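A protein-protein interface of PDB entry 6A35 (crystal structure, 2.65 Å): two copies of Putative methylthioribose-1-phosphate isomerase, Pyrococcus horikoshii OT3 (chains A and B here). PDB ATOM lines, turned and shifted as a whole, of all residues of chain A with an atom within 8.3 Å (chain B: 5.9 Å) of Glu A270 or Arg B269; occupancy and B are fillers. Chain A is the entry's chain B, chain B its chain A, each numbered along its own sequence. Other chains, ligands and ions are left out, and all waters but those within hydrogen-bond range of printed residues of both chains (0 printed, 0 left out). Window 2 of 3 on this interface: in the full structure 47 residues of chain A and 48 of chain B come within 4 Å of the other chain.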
ATOM      1  N   MET A 234     -34.292   4.474   0.435  1.00  0.00           N
ATOM      2  CA  MET A 234     -33.506   3.874  -0.620  1.00  0.00           C
ATOM      3  C   MET A 234     -34.416   3.012  -1.449  1.00  0.00           C
ATOM      4  O   MET A 234     -34.466   3.173  -2.670  1.00  0.00           O
ATOM      5  CB  MET A 234     -32.323   3.080  -0.059  1.00  0.00           C
ATOM      6  CG  MET A 234     -31.159   3.980   0.296  1.00  0.00           C
ATOM      7  SD  MET A 234     -29.762   3.068   0.964  1.00  0.00           S
ATOM      8  CE  MET A 234     -29.388   4.121   2.352  1.00  0.00           C
ATOM      9  N   GLN A 235     -35.137   2.145  -0.747  1.00  0.00           N
ATOM     10  CA  GLN A 235     -36.108   1.168  -1.292  1.00  0.00           C
ATOM     11  C   GLN A 235     -37.179   1.788  -2.181  1.00  0.00           C
ATOM     12  O   GLN A 235     -37.586   1.170  -3.156  1.00  0.00           O
ATOM     13  CB  GLN A 235     -36.801   0.394  -0.131  1.00  0.00           C
ATOM     14  CG  GLN A 235     -38.033  -0.452  -0.492  1.00  0.00           C
ATOM     15  CD  GLN A 235     -38.907  -0.875   0.708  1.00  0.00           C
ATOM     16  OE1 GLN A 235     -40.031  -0.397   0.855  1.00  0.00           O
ATOM     17  NE2 GLN A 235     -38.397  -1.780   1.553  1.00  0.00           N
ATOM     18  N   MET A 263     -23.601   0.691   7.718  1.00  0.00           N
ATOM     19  CA  MET A 263     -25.016   0.367   7.499  1.00  0.00           C
ATOM     20  C   MET A 263     -25.443   0.935   6.159  1.00  0.00           C
ATOM     21  O   MET A 263     -25.970   0.211   5.310  1.00  0.00           O
ATOM     22  CB  MET A 263     -25.884   0.935   8.646  1.00  0.00           C
ATOM     23  CG  MET A 263     -27.415   0.780   8.520  1.00  0.00           C
ATOM     24  SD  MET A 263     -28.296   2.193   7.812  1.00  0.00           S
ATOM     25  CE  MET A 263     -28.097   3.364   9.150  1.00  0.00           C
ATOM     26  N   LEU A 264     -25.172   2.216   5.954  1.00  0.00           N
ATOM     27  CA  LEU A 264     -25.471   2.855   4.670  1.00  0.00           C
ATOM     28  C   LEU A 264     -24.769   2.133   3.508  1.00  0.00           C
ATOM     29  O   LEU A 264     -25.426   1.737   2.551  1.00  0.00           O
ATOM     30  CB  LEU A 264     -25.078   4.327   4.678  1.00  0.00           C
ATOM     31  CG  LEU A 264     -25.719   5.299   5.658  1.00  0.00           C
ATOM     32  CD1 LEU A 264     -24.997   6.619   5.490  1.00  0.00           C
ATOM     33  CD2 LEU A 264     -27.193   5.496   5.388  1.00  0.00           C
ATOM     34  N   ALA A 265     -23.446   1.961   3.599  1.00  0.00           N
ATOM     35  CA  ALA A 265     -22.667   1.140   2.634  1.00  0.00           C
ATOM     36  C   ALA A 265     -23.435  -0.128   2.149  1.00  0.00           C
ATOM     37  O   ALA A 265     -23.794  -0.220   0.993  1.00  0.00           O
ATOM     38  CB  ALA A 265     -21.305   0.761   3.232  1.00  0.00           C
ATOM     39  N   VAL A 266     -23.715  -1.063   3.054  1.00  0.00           N
ATOM     40  CA  VAL A 266     -24.466  -2.301   2.746  1.00  0.00           C
ATOM     41  C   VAL A 266     -25.886  -2.089   2.150  1.00  0.00           C
ATOM     42  O   VAL A 266     -26.444  -2.956   1.465  1.00  0.00           O
ATOM     43  CB  VAL A 266     -24.565  -3.202   4.022  1.00  0.00           C
ATOM     44  CG1 VAL A 266     -25.542  -4.374   3.849  1.00  0.00           C
ATOM     45  CG2 VAL A 266     -23.182  -3.729   4.415  1.00  0.00           C
ATOM     46  N   LEU A 267     -26.490  -0.956   2.423  1.00  0.00           N
ATOM     47  CA  LEU A 267     -27.807  -0.681   1.872  1.00  0.00           C
ATOM     48  C   LEU A 267     -27.765  -0.055   0.491  1.00  0.00           C
ATOM     49  O   LEU A 267     -28.672  -0.275  -0.314  1.00  0.00           O
ATOM     50  CB  LEU A 267     -28.544   0.247   2.807  1.00  0.00           C
ATOM     51  CG  LEU A 267     -29.161  -0.459   3.983  1.00  0.00           C
ATOM     52  CD1 LEU A 267     -29.452   0.611   5.001  1.00  0.00           C
ATOM     53  CD2 LEU A 267     -30.422  -1.121   3.476  1.00  0.00           C
ATOM     54  N   ALA A 268     -26.727   0.747   0.234  1.00  0.00           N
ATOM     55  CA  ALA A 268     -26.481   1.275  -1.088  1.00  0.00           C
ATOM     56  C   ALA A 268     -26.175   0.084  -1.998  1.00  0.00           C
ATOM     57  O   ALA A 268     -26.670  -0.016  -3.139  1.00  0.00           O
ATOM     58  CB  ALA A 268     -25.308   2.230  -1.056  1.00  0.00           C
ATOM     59  N   ARG A 269     -25.363  -0.818  -1.461  1.00  0.00           N
ATOM     60  CA  ARG A 269     -25.111  -2.109  -2.050  1.00  0.00           C
ATOM     61  C   ARG A 269     -26.364  -2.813  -2.575  1.00  0.00           C
ATOM     62  O   ARG A 269     -26.400  -3.214  -3.726  1.00  0.00           O
ATOM     63  CB  ARG A 269     -24.434  -3.005  -1.021  1.00  0.00           C
ATOM     64  CG  ARG A 269     -23.042  -3.425  -1.417  1.00  0.00           C
ATOM     65  CD  ARG A 269     -22.978  -4.817  -2.022  1.00  0.00           C
ATOM     66  NE  ARG A 269     -21.803  -4.915  -2.888  1.00  0.00           N
ATOM     67  CZ  ARG A 269     -21.039  -5.993  -3.040  1.00  0.00           C
ATOM     68  NH1 ARG A 269     -19.995  -5.947  -3.866  1.00  0.00           N
ATOM     69  NH2 ARG A 269     -21.300  -7.118  -2.379  1.00  0.00           N
ATOM     70  N   GLU A 270     -27.377  -2.973  -1.733  1.00  0.00           N
ATOM     71  CA  GLU A 270     -28.498  -3.855  -2.021  1.00  0.00           C
ATOM     72  C   GLU A 270     -29.453  -3.173  -2.965  1.00  0.00           C
ATOM     73  O   GLU A 270     -30.275  -3.826  -3.550  1.00  0.00           O
ATOM     74  CB  GLU A 270     -29.228  -4.228  -0.726  1.00  0.00           C
ATOM     75  CG  GLU A 270     -30.389  -5.210  -0.865  1.00  0.00           C
ATOM     76  CD  GLU A 270     -30.073  -6.645  -0.447  1.00  0.00           C
ATOM     77  OE1 GLU A 270     -28.932  -6.945  -0.038  1.00  0.00           O
ATOM     78  OE2 GLU A 270     -30.993  -7.497  -0.521  1.00  0.00           O
ATOM     79  N   HIS A 271     -29.379  -1.856  -3.086  1.00  0.00           N
ATOM     80  CA  HIS A 271     -30.213  -1.124  -4.049  1.00  0.00           C
ATOM     81  C   HIS A 271     -29.342  -0.562  -5.182  1.00  0.00           C
ATOM     82  O   HIS A 271     -29.765   0.311  -5.929  1.00  0.00           O
ATOM     83  CB  HIS A 271     -31.003   0.001  -3.363  1.00  0.00           C
ATOM     84  CG  HIS A 271     -31.840  -0.447  -2.204  1.00  0.00           C
ATOM     85  ND1 HIS A 271     -31.353  -0.520  -0.918  1.00  0.00           N
ATOM     86  CD2 HIS A 271     -33.147  -0.800  -2.127  1.00  0.00           C
ATOM     87  CE1 HIS A 271     -32.312  -0.925  -0.102  1.00  0.00           C
ATOM     88  NE2 HIS A 271     -33.413  -1.100  -0.810  1.00  0.00           N
ATOM     89  N   GLY A 272     -28.120  -1.072  -5.303  1.00  0.00           N
ATOM     90  CA  GLY A 272     -27.198  -0.666  -6.366  1.00  0.00           C
ATOM     91  C   GLY A 272     -27.027   0.827  -6.466  1.00  0.00           C
ATOM     92  O   GLY A 272     -26.780   1.341  -7.556  1.00  0.00           O
ATOM     93  N   ILE A 273     -27.159   1.524  -5.335  1.00  0.00           N
ATOM     94  CA  ILE A 273     -26.918   2.968  -5.291  1.00  0.00           C
ATOM     95  C   ILE A 273     -25.421   3.172  -5.110  1.00  0.00           C
ATOM     96  O   ILE A 273     -24.812   2.477  -4.283  1.00  0.00           O
ATOM     97  CB  ILE A 273     -27.601   3.663  -4.097  1.00  0.00           C
ATOM     98  CG1 ILE A 273     -29.087   3.380  -4.069  1.00  0.00           C
ATOM     99  CG2 ILE A 273     -27.362   5.160  -4.161  1.00  0.00           C
ATOM    100  CD1 ILE A 273     -29.780   4.108  -2.952  1.00  0.00           C
ATOM    101  N   TYR A 330     -17.519  -1.919  -0.704  1.00  0.00           N
ATOM    102  CA  TYR A 330     -18.693  -1.044  -0.726  1.00  0.00           C
ATOM    103  C   TYR A 330     -18.487   0.349  -1.408  1.00  0.00           C
ATOM    104  O   TYR A 330     -19.465   1.004  -1.835  1.00  0.00           O
ATOM    105  CB  TYR A 330     -19.270  -0.900   0.695  1.00  0.00           C
ATOM    106  CG  TYR A 330     -19.630  -2.241   1.275  1.00  0.00           C
ATOM    107  CD1 TYR A 330     -20.723  -2.918   0.811  1.00  0.00           C
ATOM    108  CD2 TYR A 330     -18.844  -2.855   2.248  1.00  0.00           C
ATOM    109  CE1 TYR A 330     -21.061  -4.179   1.288  1.00  0.00           C
ATOM    110  CE2 TYR A 330     -19.155  -4.120   2.733  1.00  0.00           C
ATOM    111  CZ  TYR A 330     -20.263  -4.782   2.243  1.00  0.00           C
ATOM    112  OH  TYR A 330     -20.606  -6.032   2.693  1.00  0.00           O
ATOM    113  N   TYR B 262     -36.665  -2.927   7.998  1.00  0.00           N
ATOM    114  CA  TYR B 262     -36.223  -3.327   6.678  1.00  0.00           C
ATOM    115  C   TYR B 262     -34.718  -3.298   6.672  1.00  0.00           C
ATOM    116  O   TYR B 262     -34.069  -4.216   6.189  1.00  0.00           O
ATOM    117  CB  TYR B 262     -36.838  -2.455   5.559  1.00  0.00           C
ATOM    118  CG  TYR B 262     -36.232  -2.689   4.210  1.00  0.00           C
ATOM    119  CD1 TYR B 262     -36.223  -3.942   3.615  1.00  0.00           C
ATOM    120  CD2 TYR B 262     -35.684  -1.650   3.513  1.00  0.00           C
ATOM    121  CE1 TYR B 262     -35.660  -4.138   2.357  1.00  0.00           C
ATOM    122  CE2 TYR B 262     -35.118  -1.838   2.269  1.00  0.00           C
ATOM    123  CZ  TYR B 262     -35.099  -3.070   1.709  1.00  0.00           C
ATOM    124  OH  TYR B 262     -34.511  -3.154   0.497  1.00  0.00           O
ATOM    125  N   LEU B 264     -32.701  -3.821   9.014  1.00  0.00           N
ATOM    126  CA  LEU B 264     -32.185  -5.009   9.662  1.00  0.00           C
ATOM    127  C   LEU B 264     -32.240  -6.226   8.729  1.00  0.00           C
ATOM    128  O   LEU B 264     -31.273  -6.986   8.604  1.00  0.00           O
ATOM    129  CB  LEU B 264     -32.982  -5.297  10.923  1.00  0.00           C
ATOM    130  CG  LEU B 264     -32.874  -4.352  12.088  1.00  0.00           C
ATOM    131  CD1 LEU B 264     -33.920  -4.721  13.113  1.00  0.00           C
ATOM    132  CD2 LEU B 264     -31.504  -4.458  12.717  1.00  0.00           C
ATOM    133  N   ALA B 265     -33.373  -6.410   8.071  1.00  0.00           N
ATOM    134  CA  ALA B 265     -33.538  -7.554   7.229  1.00  0.00           C
ATOM    135  C   ALA B 265     -32.438  -7.610   6.157  1.00  0.00           C
ATOM    136  O   ALA B 265     -31.855  -8.673   5.935  1.00  0.00           O
ATOM    137  CB  ALA B 265     -34.918  -7.515   6.594  1.00  0.00           C
ATOM    138  N   VAL B 266     -32.183  -6.475   5.487  1.00  0.00           N
ATOM    139  CA  VAL B 266     -31.120  -6.350   4.471  1.00  0.00           C
ATOM    140  C   VAL B 266     -29.747  -6.652   5.050  1.00  0.00           C
ATOM    141  O   VAL B 266     -28.874  -7.183   4.365  1.00  0.00           O
ATOM    142  CB  VAL B 266     -31.058  -4.929   3.847  1.00  0.00           C
ATOM    143  CG1 VAL B 266     -29.766  -4.719   3.066  1.00  0.00           C
ATOM    144  CG2 VAL B 266     -32.245  -4.686   2.918  1.00  0.00           C
ATOM    145  N   LEU B 267     -29.540  -6.274   6.306  1.00  0.00           N
ATOM    146  CA  LEU B 267     -28.247  -6.500   6.962  1.00  0.00           C
ATOM    147  C   LEU B 267     -28.107  -7.917   7.463  1.00  0.00           C
ATOM    148  O   LEU B 267     -26.997  -8.480   7.436  1.00  0.00           O
ATOM    149  CB  LEU B 267     -28.074  -5.539   8.126  1.00  0.00           C
ATOM    150  CG  LEU B 267     -27.911  -4.086   7.713  1.00  0.00           C
ATOM    151  CD1 LEU B 267     -28.059  -3.258   8.970  1.00  0.00           C
ATOM    152  CD2 LEU B 267     -26.575  -3.862   7.080  1.00  0.00           C
ATOM    153  N   ALA B 268     -29.237  -8.453   7.935  1.00  0.00           N
ATOM    154  CA  ALA B 268     -29.296  -9.780   8.491  1.00  0.00           C
ATOM    155  C   ALA B 268     -28.952 -10.735   7.372  1.00  0.00           C
ATOM    156  O   ALA B 268     -28.357 -11.818   7.602  1.00  0.00           O
ATOM    157  CB  ALA B 268     -30.685 -10.064   9.017  1.00  0.00           C
ATOM    158  N   ARG B 269     -29.328 -10.265   6.166  1.00  0.00           N
ATOM    159  CA  ARG B 269     -29.155 -10.939   4.894  1.00  0.00           C
ATOM    160  C   ARG B 269     -27.747 -10.873   4.358  1.00  0.00           C
ATOM    161  O   ARG B 269     -27.300 -11.805   3.744  1.00  0.00           O
ATOM    162  CB  ARG B 269     -30.094 -10.326   3.858  1.00  0.00           C
ATOM    163  CG  ARG B 269     -30.818 -11.366   3.050  1.00  0.00           C
ATOM    164  CD  ARG B 269     -30.498 -11.289   1.583  1.00  0.00           C
ATOM    165  NE  ARG B 269     -31.332 -12.248   0.854  1.00  0.00           N
ATOM    166  CZ  ARG B 269     -31.475 -12.279  -0.461  1.00  0.00           C
ATOM    167  NH1 ARG B 269     -32.249 -13.205  -1.005  1.00  0.00           N
ATOM    168  NH2 ARG B 269     -30.847 -11.392  -1.234  1.00  0.00           N
ATOM    169  N   GLU B 270     -27.054  -9.768   4.570  1.00  0.00           N
ATOM    170  CA  GLU B 270     -25.659  -9.647   4.131  1.00  0.00           C
ATOM    171  C   GLU B 270     -24.684 -10.494   4.972  1.00  0.00           C
ATOM    172  O   GLU B 270     -23.632 -10.869   4.488  1.00  0.00           O
ATOM    173  CB  GLU B 270     -25.213  -8.183   4.168  1.00  0.00           C
ATOM    174  CG  GLU B 270     -23.767  -7.916   3.724  1.00  0.00           C
ATOM    175  CD  GLU B 270     -23.636  -7.409   2.302  1.00  0.00           C
ATOM    176  OE1 GLU B 270     -24.650  -7.418   1.545  1.00  0.00           O
ATOM    177  OE2 GLU B 270     -22.505  -6.991   1.942  1.00  0.00           O
ATOM    178  N   HIS B 271     -25.017 -10.764   6.227  1.00  0.00           N
ATOM    179  CA  HIS B 271     -24.134 -11.544   7.101  1.00  0.00           C
ATOM    180  C   HIS B 271     -24.735 -12.924   7.341  1.00  0.00           C
ATOM    181  O   HIS B 271     -24.410 -13.581   8.329  1.00  0.00           O
ATOM    182  CB  HIS B 271     -23.905 -10.836   8.445  1.00  0.00           C
ATOM    183  CG  HIS B 271     -23.512  -9.393   8.318  1.00  0.00           C
ATOM    184  ND1 HIS B 271     -24.432  -8.377   8.146  1.00  0.00           N
ATOM    185  CD2 HIS B 271     -22.298  -8.797   8.350  1.00  0.00           C
ATOM    186  CE1 HIS B 271     -23.798  -7.221   8.060  1.00  0.00           C
ATOM    187  NE2 HIS B 271     -22.504  -7.447   8.186  1.00  0.00           N
ATOM    188  N   GLY B 272     -25.630 -13.342   6.452  1.00  0.00           N
ATOM    189  CA  GLY B 272     -26.266 -14.639   6.564  1.00  0.00           C
ATOM    190  C   GLY B 272     -26.727 -14.939   7.968  1.00  0.00           C
ATOM    191  O   GLY B 272     -26.524 -16.033   8.456  1.00  0.00           O
ATOM    192  N   ILE B 273     -27.338 -13.946   8.594  1.00  0.00           N
ATOM    193  CA  ILE B 273     -27.925 -14.064   9.920  1.00  0.00           C
ATOM    194  C   ILE B 273     -29.435 -14.296   9.740  1.00  0.00           C
ATOM    195  O   ILE B 273     -30.109 -13.544   9.023  1.00  0.00           O
ATOM    196  CB  ILE B 273     -27.735 -12.777  10.767  1.00  0.00           C
ATOM    197  CG1 ILE B 273     -26.320 -12.660  11.312  1.00  0.00           C
ATOM    198  CG2 ILE B 273     -28.692 -12.770  11.956  1.00  0.00           C
ATOM    199  CD1 ILE B 273     -26.012 -11.288  11.853  1.00  0.00           C
ATOM    200  N   LYS B 329     -38.798 -12.143   0.855  1.00  0.00           N
ATOM    201  CA  LYS B 329     -37.559 -12.864   0.601  1.00  0.00           C
ATOM    202  C   LYS B 329     -36.506 -12.776   1.702  1.00  0.00           C
ATOM    203  O   LYS B 329     -35.620 -13.601   1.719  1.00  0.00           O
ATOM    204  CB  LYS B 329     -36.916 -12.473  -0.727  1.00  0.00           C
ATOM    205  CG  LYS B 329     -36.214 -11.143  -0.777  1.00  0.00           C
ATOM    206  CD  LYS B 329     -35.314 -11.116  -1.996  1.00  0.00           C
ATOM    207  CE  LYS B 329     -34.783  -9.717  -2.289  1.00  0.00           C
ATOM    208  NZ  LYS B 329     -33.798  -9.672  -3.416  1.00  0.00           N
ATOM    209  N   TYR B 330     -36.608 -11.790   2.598  1.00  0.00           N
ATOM    210  CA  TYR B 330     -35.647 -11.625   3.695  1.00  0.00           C
ATOM    211  C   TYR B 330     -36.045 -12.407   4.923  1.00  0.00           C
ATOM    212  O   TYR B 330     -35.306 -12.454   5.896  1.00  0.00           O
ATOM    213  CB  TYR B 330     -35.488 -10.150   4.070  1.00  0.00           C
ATOM    214  CG  TYR B 330     -34.916  -9.327   2.934  1.00  0.00           C
ATOM    215  CD1 TYR B 330     -33.565  -9.272   2.723  1.00  0.00           C
ATOM    216  CD2 TYR B 330     -35.755  -8.637   2.063  1.00  0.00           C
ATOM    217  CE1 TYR B 330     -33.037  -8.539   1.686  1.00  0.00           C
ATOM    218  CE2 TYR B 330     -35.253  -7.880   1.015  1.00  0.00           C
ATOM    219  CZ  TYR B 330     -33.894  -7.824   0.817  1.00  0.00           C
ATOM    220  OH  TYR B 330     -33.388  -7.083  -0.230  1.00  0.00           O
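A ring nitrogen (NE2) of His A271 is in hydrogen-bond range of the side-chain hydroxyl of Tyr B262 (2.7 Å). OE2 of Glu B270 lies close to OH of Tyr A330 (2.3 Å). The side-chain carboxylate (OE2) of Glu A270 is in hydrogen-bond range of the side-chain hydroxyl (OH) of Tyr B330. NH2 of Arg B269 lies within salt-bridge range of OE2 of Glu A270 (3.96 Å).
Along chain A the printed residues that touch a printed residue of chain B span positions 235 to 330. Hydrophobic or aromatic side chains of chain B that line the printed part of chain A: Tyr B262, Val B266, Leu B267 and Tyr B330. Among the printed residues, Asp or Glu carboxylates within 4 Å of a Lys or Arg side-chain nitrogen of the other chain: Glu A270 with Arg B269.
Val A266 touches Leu B267, and with the chains exchanged Leu A267 touches Val B266. Val A266 touches Glu B270, and with the chains exchanged Glu A270 touches Val B266. Glu A270 touches Arg B269, but with the chains exchanged Arg A269 does not touch Glu B270 (4.5 Å). Glu A270 touches Tyr B330, and with the chains exchanged Tyr A330 touches Glu B270. Of the 9 pairs that touch across the chains among the printed residues, 6 have their exchanged pair printed and touching as well.
Printed residues of chain B within 4 Å of Val A266: Leu B267 (3.4 Å) and Glu B270 (3.8 Å). Printed residues of chain B within 4 Å of His A271: Tyr B262. Gly A272 touches none of the printed residues of chain B. Of the printed residues of chain B, Tyr A330 touches Glu B270 (2.3 Å). No residue of chain A comes within 4 Å of Ala B268. Printed residues of chain A within 4 Å of Arg B269: Glu A270 (3.96 Å). Printed residues of chain A within 4 Å of Glu B270: Val A266 and Tyr A330. Ile B273 touches none of the printed residues of chain A. Printed residues of chain A within 4 Å of Tyr B330: Glu A270 (2.4 Å). The nearest printed residue of chain A that does not touch Tyr B330 is His A271 (6.0 Å).
O of Leu B267 is in hydrogen-bond range of ND1 of His B271. The backbone carbonyl oxygen (O) of Leu A267 sits at hydrogen-bond distance from a ring nitrogen (ND1) of His A271, 2.8 Å away.
Among the printed residues, pairs that only touch across the chains: Gln A235 with Tyr B262 (3.3 Å), Val A266 with Leu B267 (3.4 Å), Val A266 with Glu B270 (3.8 Å), Leu A267 with Val B266 (3.7 Å) and Glu A270 with Val B266 (3.9 Å).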
